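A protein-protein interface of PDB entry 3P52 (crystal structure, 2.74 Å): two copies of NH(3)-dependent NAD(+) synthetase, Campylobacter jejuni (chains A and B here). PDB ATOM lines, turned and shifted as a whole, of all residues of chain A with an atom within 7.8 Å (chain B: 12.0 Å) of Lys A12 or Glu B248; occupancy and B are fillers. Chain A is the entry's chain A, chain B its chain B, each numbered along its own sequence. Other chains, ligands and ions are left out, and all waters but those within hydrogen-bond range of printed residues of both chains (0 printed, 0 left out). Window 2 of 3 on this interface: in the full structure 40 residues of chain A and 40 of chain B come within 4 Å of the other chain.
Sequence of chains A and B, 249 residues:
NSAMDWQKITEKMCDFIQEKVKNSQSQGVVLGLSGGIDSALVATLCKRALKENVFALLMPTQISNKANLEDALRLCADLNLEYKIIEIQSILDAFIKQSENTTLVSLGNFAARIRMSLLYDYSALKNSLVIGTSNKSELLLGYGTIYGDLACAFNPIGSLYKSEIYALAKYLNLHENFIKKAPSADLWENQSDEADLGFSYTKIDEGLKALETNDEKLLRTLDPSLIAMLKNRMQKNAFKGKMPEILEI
Of chain B, only Leu B247 (3.9 Å) and Glu B248 (3.8 Å) come within 4 Å of Lys A12. Printed residues of chain A within 4 Å of Glu B248: Lys A12. No residue of chain B comes within 4 Å of Ile A9. No residue of chain B comes within 4 Å of Glu A11. Met A13 touches just one residue of chain B: Leu B247. No residue of chain B comes within 4 Å of Asp A15. Phe A16 touches two residues of chain B. Gly A158 touches just one residue of chain B: Ile B246. Of the printed residues of chain A, Ile B246 touches Asn A155 (3.5 Å) and Gly A158 (3.9 Å). Of the printed residues of chain B, Ser A159 touches Leu B247. Printed residues of chain A within 4 Å of Glu B245: Phe A16 and Asn A155. Of the printed residues of chain A, Leu B247 touches Lys A12 (3.9 Å), Met A13 (3.8 Å), Phe A16 (3.3 Å), Asn A155 (3.4 Å) and Ser A159 (3.9 Å). Pro B244 touches none of the printed residues of chain A.
No position is printed for both chains. Of the 10 pairs that touch across the chains among the printed residues, none has its exchanged pair printed and touching as well.
OD1 of Asn A155 is in hydrogen-bond range of N of Gly A158, 3.0 Å away.
O of Lys A12 touches CD2 of Leu B247, at 3.9 Å. Glu B248 touches Lys A12 (C to NZ, 3.8 Å). Leu B247 touches Met A13 (CD2 to CG, 3.8 Å). O of Glu B245 touches CZ of Phe A16, 3.5 Å away. CD1 of Leu B247 touches CD1 of Phe A16, at 3.3 Å. O of Asn A155 touches CA of Ile B246, at 3.5 Å. Gly A158 touches Ile B246. Ser A159 touches Leu B247.
Of the 23 printed residues of chain A, 6 touch a printed residue of chain B. Printed residues of chain B that touch a printed residue of chain A: Glu B245, Ile B246, Leu B247 and Glu B248. Among the printed residues, 10 pairs touch across the chains. Among the printed residues, no Asp or Glu carboxylate lies within 4 Å of a Lys or Arg side-chain nitrogen of the other chain.
The backbone carbonyl oxygen (O) of Asn A155 sits at hydrogen-bond distance from the backbone NH (N) of Leu B247 (3.4 Å). The backbone NH (N) of Asn A155 lies within hydrogen-bond range of the backbone carbonyl oxygen (O) of Glu B245 (3.3 Å).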
ATOM      1  N   ASP A   5      19.049  16.512 -38.437  1.00  0.00           N
ATOM      2  CA  ASP A   5      17.937  17.007 -37.633  1.00  0.00           C
ATOM      3  C   ASP A   5      18.193  16.958 -36.125  1.00  0.00           C
ATOM      4  O   ASP A   5      17.855  15.975 -35.452  1.00  0.00           O
ATOM      5  CB  ASP A   5      16.642  16.270 -37.991  1.00  0.00           C
ATOM      6  CG  ASP A   5      15.411  16.893 -37.340  1.00  0.00           C
ATOM      7  OD1 ASP A   5      15.544  17.925 -36.636  1.00  0.00           O
ATOM      8  OD2 ASP A   5      14.311  16.333 -37.528  1.00  0.00           O
ATOM      9  N   TRP A   6      18.762  18.037 -35.592  1.00  0.00           N
ATOM     10  CA  TRP A   6      19.196  18.064 -34.196  1.00  0.00           C
ATOM     11  C   TRP A   6      18.049  18.014 -33.222  1.00  0.00           C
ATOM     12  O   TRP A   6      18.157  17.363 -32.192  1.00  0.00           O
ATOM     13  CB  TRP A   6      20.073  19.276 -33.915  1.00  0.00           C
ATOM     14  CG  TRP A   6      21.258  19.340 -34.806  1.00  0.00           C
ATOM     15  CD1 TRP A   6      21.588  20.350 -35.653  1.00  0.00           C
ATOM     16  CD2 TRP A   6      22.271  18.336 -34.968  1.00  0.00           C
ATOM     17  NE1 TRP A   6      22.753  20.049 -36.320  1.00  0.00           N
ATOM     18  CE2 TRP A   6      23.191  18.820 -35.916  1.00  0.00           C
ATOM     19  CE3 TRP A   6      22.497  17.080 -34.389  1.00  0.00           C
ATOM     20  CZ2 TRP A   6      24.305  18.098 -36.305  1.00  0.00           C
ATOM     21  CZ3 TRP A   6      23.611  16.363 -34.774  1.00  0.00           C
ATOM     22  CH2 TRP A   6      24.502  16.874 -35.720  1.00  0.00           C
ATOM     23  N   GLN A   7      16.955  18.690 -33.552  1.00  0.00           N
ATOM     24  CA  GLN A   7      15.775  18.696 -32.699  1.00  0.00           C
ATOM     25  C   GLN A   7      15.302  17.266 -32.466  1.00  0.00           C
ATOM     26  O   GLN A   7      14.983  16.889 -31.340  1.00  0.00           O
ATOM     27  CB  GLN A   7      14.667  19.535 -33.329  1.00  0.00           C
ATOM     28  CG  GLN A   7      13.469  19.829 -32.425  1.00  0.00           C
ATOM     29  CD  GLN A   7      12.398  20.682 -33.125  1.00  0.00           C
ATOM     30  OE1 GLN A   7      11.982  20.395 -34.257  1.00  0.00           O
ATOM     31  NE2 GLN A   7      11.955  21.739 -32.450  1.00  0.00           N
ATOM     32  N   LYS A   8      15.280  16.474 -33.534  1.00  0.00           N
ATOM     33  CA  LYS A   8      14.831  15.096 -33.451  1.00  0.00           C
ATOM     34  C   LYS A   8      15.885  14.240 -32.752  1.00  0.00           C
ATOM     35  O   LYS A   8      15.560  13.374 -31.941  1.00  0.00           O
ATOM     36  CB  LYS A   8      14.505  14.548 -34.847  1.00  0.00           C
ATOM     37  CG  LYS A   8      13.777  13.210 -34.848  1.00  0.00           C
ATOM     38  CD  LYS A   8      13.835  12.545 -36.220  1.00  0.00           C
ATOM     39  CE  LYS A   8      13.654  11.023 -36.105  1.00  0.00           C
ATOM     40  NZ  LYS A   8      13.630  10.320 -37.425  1.00  0.00           N
ATOM     41  N   ILE A   9      17.151  14.491 -33.058  1.00  0.00           N
ATOM     42  CA  ILE A   9      18.236  13.776 -32.402  1.00  0.00           C
ATOM     43  C   ILE A   9      18.232  14.019 -30.887  1.00  0.00           C
ATOM     44  O   ILE A   9      18.339  13.072 -30.106  1.00  0.00           O
ATOM     45  CB  ILE A   9      19.598  14.052 -33.091  1.00  0.00           C
ATOM     46  CG1 ILE A   9      19.792  13.048 -34.235  1.00  0.00           C
ATOM     47  CG2 ILE A   9      20.776  13.936 -32.128  1.00  0.00           C
ATOM     48  CD1 ILE A   9      20.979  13.329 -35.149  1.00  0.00           C
ATOM     49  N   THR A  10      18.052  15.272 -30.483  1.00  0.00           N
ATOM     50  CA  THR A  10      17.977  15.621 -29.075  1.00  0.00           C
ATOM     51  C   THR A  10      16.864  14.877 -28.359  1.00  0.00           C
ATOM     52  O   THR A  10      17.069  14.325 -27.290  1.00  0.00           O
ATOM     53  CB  THR A  10      17.800  17.123 -28.887  1.00  0.00           C
ATOM     54  OG1 THR A  10      18.996  17.785 -29.289  1.00  0.00           O
ATOM     55  CG2 THR A  10      17.547  17.465 -27.443  1.00  0.00           C
ATOM     56  N   GLU A  11      15.685  14.850 -28.955  1.00  0.00           N
ATOM     57  CA  GLU A  11      14.536  14.222 -28.319  1.00  0.00           C
ATOM     58  C   GLU A  11      14.767  12.711 -28.218  1.00  0.00           C
ATOM     59  O   GLU A  11      14.422  12.070 -27.215  1.00  0.00           O
ATOM     60  CB  GLU A  11      13.263  14.542 -29.096  1.00  0.00           C
ATOM     61  CG  GLU A  11      12.019  14.761 -28.237  1.00  0.00           C
ATOM     62  CD  GLU A  11      10.741  14.930 -29.086  1.00  0.00           C
ATOM     63  OE1 GLU A  11      10.850  15.179 -30.313  1.00  0.00           O
ATOM     64  OE2 GLU A  11       9.627  14.816 -28.527  1.00  0.00           O
ATOM     65  N   LYS A  12      15.396  12.155 -29.245  1.00  0.00           N
ATOM     66  CA  LYS A  12      15.705  10.736 -29.253  1.00  0.00           C
ATOM     67  C   LYS A  12      16.610  10.380 -28.082  1.00  0.00           C
ATOM     68  O   LYS A  12      16.413   9.360 -27.421  1.00  0.00           O
ATOM     69  CB  LYS A  12      16.345  10.340 -30.584  1.00  0.00           C
ATOM     70  CG  LYS A  12      16.040   8.920 -30.998  1.00  0.00           C
ATOM     71  CD  LYS A  12      15.958   8.799 -32.522  1.00  0.00           C
ATOM     72  CE  LYS A  12      15.802   7.332 -32.967  1.00  0.00           C
ATOM     73  NZ  LYS A  12      16.880   6.454 -32.366  1.00  0.00           N
ATOM     74  N   MET A  13      17.584  11.250 -27.828  1.00  0.00           N
ATOM     75  CA  MET A  13      18.578  11.069 -26.763  1.00  0.00           C
ATOM     76  C   MET A  13      17.982  11.195 -25.379  1.00  0.00           C
ATOM     77  O   MET A  13      18.273  10.389 -24.506  1.00  0.00           O
ATOM     78  CB  MET A  13      19.718  12.050 -26.935  1.00  0.00           C
ATOM     79  CG  MET A  13      20.589  11.668 -28.089  1.00  0.00           C
ATOM     80  SD  MET A  13      22.050  12.933 -28.474  1.00  0.00           S
ATOM     81  CE  MET A  13      23.167  11.814 -29.640  1.00  0.00           C
ATOM     82  N   CYS A  14      17.130  12.194 -25.188  1.00  0.00           N
ATOM     83  CA  CYS A  14      16.426  12.339 -23.935  1.00  0.00           C
ATOM     84  C   CYS A  14      15.551  11.136 -23.642  1.00  0.00           C
ATOM     85  O   CYS A  14      15.562  10.643 -22.523  1.00  0.00           O
ATOM     86  CB  CYS A  14      15.637  13.635 -23.907  1.00  0.00           C
ATOM     87  SG  CYS A  14      16.723  15.069 -23.956  1.00  0.00           S
ATOM     88  N   ASP A  15      14.821  10.648 -24.645  1.00  0.00           N
ATOM     89  CA  ASP A  15      14.021   9.436 -24.490  1.00  0.00           C
ATOM     90  C   ASP A  15      14.863   8.305 -23.950  1.00  0.00           C
ATOM     91  O   ASP A  15      14.497   7.652 -22.972  1.00  0.00           O
ATOM     92  CB  ASP A  15      13.412   8.994 -25.824  1.00  0.00           C
ATOM     93  CG  ASP A  15      12.113   9.697 -26.130  1.00  0.00           C
ATOM     94  OD1 ASP A  15      11.639  10.476 -25.266  1.00  0.00           O
ATOM     95  OD2 ASP A  15      11.567   9.472 -27.239  1.00  0.00           O
ATOM     96  N   PHE A  16      15.997   8.090 -24.610  1.00  0.00           N
ATOM     97  CA  PHE A  16      16.920   7.013 -24.295  1.00  0.00           C
ATOM     98  C   PHE A  16      17.437   7.098 -22.856  1.00  0.00           C
ATOM     99  O   PHE A  16      17.484   6.096 -22.147  1.00  0.00           O
ATOM    100  CB  PHE A  16      18.075   7.082 -25.276  1.00  0.00           C
ATOM    101  CG  PHE A  16      19.151   6.077 -25.033  1.00  0.00           C
ATOM    102  CD1 PHE A  16      18.961   4.746 -25.398  1.00  0.00           C
ATOM    103  CD2 PHE A  16      20.375   6.470 -24.476  1.00  0.00           C
ATOM    104  CE1 PHE A  16      19.964   3.805 -25.216  1.00  0.00           C
ATOM    105  CE2 PHE A  16      21.391   5.532 -24.278  1.00  0.00           C
ATOM    106  CZ  PHE A  16      21.180   4.187 -24.654  1.00  0.00           C
ATOM    107  N   ILE A  17      17.823   8.296 -22.432  1.00  0.00           N
ATOM    108  CA  ILE A  17      18.287   8.512 -21.078  1.00  0.00           C
ATOM    109  C   ILE A  17      17.167   8.161 -20.083  1.00  0.00           C
ATOM    110  O   ILE A  17      17.383   7.364 -19.168  1.00  0.00           O
ATOM    111  CB  ILE A  17      18.820   9.951 -20.901  1.00  0.00           C
ATOM    112  CG1 ILE A  17      20.141  10.108 -21.637  1.00  0.00           C
ATOM    113  CG2 ILE A  17      19.034  10.267 -19.464  1.00  0.00           C
ATOM    114  CD1 ILE A  17      20.420  11.515 -22.115  1.00  0.00           C
ATOM    115  N   GLN A  18      15.972   8.729 -20.283  1.00  0.00           N
ATOM    116  CA  GLN A  18      14.815   8.438 -19.443  1.00  0.00           C
ATOM    117  C   GLN A  18      14.483   6.955 -19.400  1.00  0.00           C
ATOM    118  O   GLN A  18      14.139   6.424 -18.346  1.00  0.00           O
ATOM    119  CB  GLN A  18      13.601   9.207 -19.931  1.00  0.00           C
ATOM    120  CG  GLN A  18      13.643  10.685 -19.660  1.00  0.00           C
ATOM    121  CD  GLN A  18      12.560  11.422 -20.404  1.00  0.00           C
ATOM    122  OE1 GLN A  18      11.399  11.075 -20.295  1.00  0.00           O
ATOM    123  NE2 GLN A  18      12.930  12.438 -21.166  1.00  0.00           N
ATOM    124  N   GLU A  19      14.599   6.299 -20.548  1.00  0.00           N
ATOM    125  CA  GLU A  19      14.323   4.876 -20.669  1.00  0.00           C
ATOM    126  C   GLU A  19      15.270   4.027 -19.830  1.00  0.00           C
ATOM    127  O   GLU A  19      14.843   3.035 -19.261  1.00  0.00           O
ATOM    128  CB  GLU A  19      14.369   4.426 -22.139  1.00  0.00           C
ATOM    129  CG  GLU A  19      13.022   4.439 -22.915  1.00  0.00           C
ATOM    130  CD  GLU A  19      13.218   4.627 -24.444  1.00  0.00           C
ATOM    131  OE1 GLU A  19      12.311   5.176 -25.105  1.00  0.00           O
ATOM    132  OE2 GLU A  19      14.291   4.255 -24.991  1.00  0.00           O
ATOM    133  N   LEU A  45      22.213  17.315 -21.704  1.00  0.00           N
ATOM    134  CA  LEU A  45      21.087  16.481 -22.110  1.00  0.00           C
ATOM    135  C   LEU A  45      20.468  15.896 -20.882  1.00  0.00           C
ATOM    136  O   LEU A  45      19.255  15.945 -20.722  1.00  0.00           O
ATOM    137  CB  LEU A  45      21.487  15.374 -23.070  1.00  0.00           C
ATOM    138  CG  LEU A  45      21.957  15.812 -24.446  1.00  0.00           C
ATOM    139  CD1 LEU A  45      22.731  14.667 -25.138  1.00  0.00           C
ATOM    140  CD2 LEU A  45      20.793  16.277 -25.255  1.00  0.00           C
ATOM    141  N   ARG A  48      18.103  18.132 -19.070  1.00  0.00           N
ATOM    142  CA  ARG A  48      16.848  18.235 -19.821  1.00  0.00           C
ATOM    143  C   ARG A  48      15.993  16.989 -19.598  1.00  0.00           C
ATOM    144  O   ARG A  48      14.810  17.086 -19.354  1.00  0.00           O
ATOM    145  CB  ARG A  48      17.114  18.405 -21.317  1.00  0.00           C
ATOM    146  CG  ARG A  48      17.110  19.850 -21.838  1.00  0.00           C
ATOM    147  CD  ARG A  48      17.018  19.870 -23.388  1.00  0.00           C
ATOM    148  NE  ARG A  48      15.875  19.078 -23.852  1.00  0.00           N
ATOM    149  CZ  ARG A  48      15.349  19.137 -25.077  1.00  0.00           C
ATOM    150  NH1 ARG A  48      15.876  19.948 -25.995  1.00  0.00           N
ATOM    151  NH2 ARG A  48      14.294  18.375 -25.393  1.00  0.00           N
ATOM    152  N   LYS A 136      31.953   8.733 -31.050  1.00  0.00           N
ATOM    153  CA  LYS A 136      32.241   7.629 -31.971  1.00  0.00           C
ATOM    154  C   LYS A 136      33.660   7.670 -32.512  1.00  0.00           C
ATOM    155  O   LYS A 136      34.266   6.615 -32.722  1.00  0.00           O
ATOM    156  CB  LYS A 136      31.250   7.594 -33.131  1.00  0.00           C
ATOM    157  CG  LYS A 136      31.172   6.240 -33.845  1.00  0.00           C
ATOM    158  CD  LYS A 136      30.479   6.381 -35.208  1.00  0.00           C
ATOM    159  CE  LYS A 136      30.180   5.025 -35.880  1.00  0.00           C
ATOM    160  NZ  LYS A 136      28.816   4.468 -35.533  1.00  0.00           N
ATOM    161  N   ASN A 155      25.604   5.181 -22.882  1.00  0.00           N
ATOM    162  CA  ASN A 155      26.233   6.319 -23.523  1.00  0.00           C
ATOM    163  C   ASN A 155      25.353   6.853 -24.677  1.00  0.00           C
ATOM    164  O   ASN A 155      25.242   6.217 -25.738  1.00  0.00           O
ATOM    165  CB  ASN A 155      27.593   5.869 -24.063  1.00  0.00           C
ATOM    166  CG  ASN A 155      28.295   6.938 -24.843  1.00  0.00           C
ATOM    167  OD1 ASN A 155      27.741   8.000 -25.133  1.00  0.00           O
ATOM    168  ND2 ASN A 155      29.524   6.668 -25.194  1.00  0.00           N
ATOM    169  N   PRO A 156      24.755   8.036 -24.502  1.00  0.00           N
ATOM    170  CA  PRO A 156      23.874   8.599 -25.540  1.00  0.00           C
ATOM    171  C   PRO A 156      24.603   9.087 -26.793  1.00  0.00           C
ATOM    172  O   PRO A 156      23.976   9.202 -27.864  1.00  0.00           O
ATOM    173  CB  PRO A 156      23.247   9.801 -24.853  1.00  0.00           C
ATOM    174  CG  PRO A 156      24.291  10.214 -23.828  1.00  0.00           C
ATOM    175  CD  PRO A 156      24.935   8.948 -23.362  1.00  0.00           C
ATOM    176  N   GLY A 158      27.620   7.990 -28.123  1.00  0.00           N
ATOM    177  CA  GLY A 158      28.650   7.121 -28.677  1.00  0.00           C
ATOM    178  C   GLY A 158      28.616   6.861 -30.173  1.00  0.00           C
ATOM    179  O   GLY A 158      29.486   6.183 -30.692  1.00  0.00           O
ATOM    180  N   SER A 159      27.619   7.382 -30.878  1.00  0.00           N
ATOM    181  CA  SER A 159      27.506   7.110 -32.318  1.00  0.00           C
ATOM    182  C   SER A 159      27.655   8.394 -33.132  1.00  0.00           C
ATOM    183  O   SER A 159      27.540   8.380 -34.367  1.00  0.00           O
ATOM    184  CB  SER A 159      26.158   6.474 -32.645  1.00  0.00           C
ATOM    185  OG  SER A 159      25.237   7.514 -32.947  1.00  0.00           O
ATOM    186  N   LEU A 160      27.883   9.499 -32.425  1.00  0.00           N
ATOM    187  CA  LEU A 160      28.056  10.785 -33.059  1.00  0.00           C
ATOM    188  C   LEU A 160      29.544  10.987 -33.211  1.00  0.00           C
ATOM    189  O   LEU A 160      30.271  10.751 -32.263  1.00  0.00           O
ATOM    190  CB  LEU A 160      27.431  11.898 -32.209  1.00  0.00           C
ATOM    191  CG  LEU A 160      26.064  12.421 -32.655  1.00  0.00           C
ATOM    192  CD1 LEU A 160      25.052  11.315 -32.896  1.00  0.00           C
ATOM    193  CD2 LEU A 160      25.539  13.331 -31.592  1.00  0.00           C
ATOM    194  N   MET B 243      28.289  -5.301 -22.521  1.00  0.00           N
ATOM    195  CA  MET B 243      28.887  -3.997 -22.821  1.00  0.00           C
ATOM    196  C   MET B 243      27.899  -2.877 -22.542  1.00  0.00           C
ATOM    197  O   MET B 243      26.688  -3.113 -22.474  1.00  0.00           O
ATOM    198  CB  MET B 243      29.249  -3.920 -24.305  1.00  0.00           C
ATOM    199  CG  MET B 243      30.429  -4.770 -24.730  1.00  0.00           C
ATOM    200  SD  MET B 243      32.167  -4.045 -24.144  1.00  0.00           S
ATOM    201  CE  MET B 243      32.165  -2.310 -25.096  1.00  0.00           C
ATOM    202  N   PRO B 244      28.403  -1.644 -22.408  1.00  0.00           N
ATOM    203  CA  PRO B 244      27.483  -0.533 -22.293  1.00  0.00           C
ATOM    204  C   PRO B 244      26.603  -0.411 -23.524  1.00  0.00           C
ATOM    205  O   PRO B 244      27.083  -0.585 -24.640  1.00  0.00           O
ATOM    206  CB  PRO B 244      28.409   0.678 -22.188  1.00  0.00           C
ATOM    207  CG  PRO B 244      29.718   0.211 -22.676  1.00  0.00           C
ATOM    208  CD  PRO B 244      29.797  -1.206 -22.264  1.00  0.00           C
ATOM    209  N   GLU B 245      25.327  -0.111 -23.312  1.00  0.00           N
ATOM    210  CA  GLU B 245      24.418   0.102 -24.413  1.00  0.00           C
ATOM    211  C   GLU B 245      24.526   1.521 -24.941  1.00  0.00           C
ATOM    212  O   GLU B 245      24.246   2.480 -24.238  1.00  0.00           O
ATOM    213  CB  GLU B 245      22.981  -0.228 -24.012  1.00  0.00           C
ATOM    214  CG  GLU B 245      21.956   0.183 -25.069  1.00  0.00           C
ATOM    215  CD  GLU B 245      20.819  -0.814 -25.266  1.00  0.00           C
ATOM    216  OE1 GLU B 245      20.984  -2.013 -24.920  1.00  0.00           O
ATOM    217  OE2 GLU B 245      19.762  -0.384 -25.791  1.00  0.00           O
ATOM    218  N   ILE B 246      24.942   1.629 -26.194  1.00  0.00           N
ATOM    219  CA  ILE B 246      25.014   2.893 -26.913  1.00  0.00           C
ATOM    220  C   ILE B 246      23.758   3.118 -27.758  1.00  0.00           C
ATOM    221  O   ILE B 246      23.363   2.242 -28.512  1.00  0.00           O
ATOM    222  CB  ILE B 246      26.240   2.888 -27.833  1.00  0.00           C
ATOM    223  CG1 ILE B 246      27.514   2.827 -26.993  1.00  0.00           C
ATOM    224  CG2 ILE B 246      26.253   4.096 -28.745  1.00  0.00           C
ATOM    225  CD1 ILE B 246      28.681   2.211 -27.690  1.00  0.00           C
ATOM    226  N   LEU B 247      23.141   4.289 -27.629  1.00  0.00           N
ATOM    227  CA  LEU B 247      21.962   4.638 -28.404  1.00  0.00           C
ATOM    228  C   LEU B 247      22.311   4.794 -29.876  1.00  0.00           C
ATOM    229  O   LEU B 247      23.362   5.338 -30.194  1.00  0.00           O
ATOM    230  CB  LEU B 247      21.342   5.940 -27.897  1.00  0.00           C
ATOM    231  CG  LEU B 247      20.174   6.520 -28.717  1.00  0.00           C
ATOM    232  CD1 LEU B 247      18.878   5.731 -28.535  1.00  0.00           C
ATOM    233  CD2 LEU B 247      19.953   7.984 -28.409  1.00  0.00           C
ATOM    234  N   GLU B 248      21.420   4.328 -30.758  1.00  0.00           N
ATOM    235  CA  GLU B 248      21.549   4.486 -32.219  1.00  0.00           C
ATOM    236  C   GLU B 248      20.507   5.439 -32.811  1.00  0.00           C
ATOM    237  O   GLU B 248      20.850   6.413 -33.474  1.00  0.00           O
ATOM    238  CB  GLU B 248      21.437   3.124 -32.903  1.00  0.00           C
ATOM    239  CG  GLU B 248      22.603   2.173 -32.609  1.00  0.00           C
ATOM    240  CD  GLU B 248      23.895   2.530 -33.372  1.00  0.00           C
ATOM    241  OE1 GLU B 248      23.833   2.685 -34.621  1.00  0.00           O
ATOM    242  OE2 GLU B 248      24.976   2.642 -32.721  1.00  0.00           O
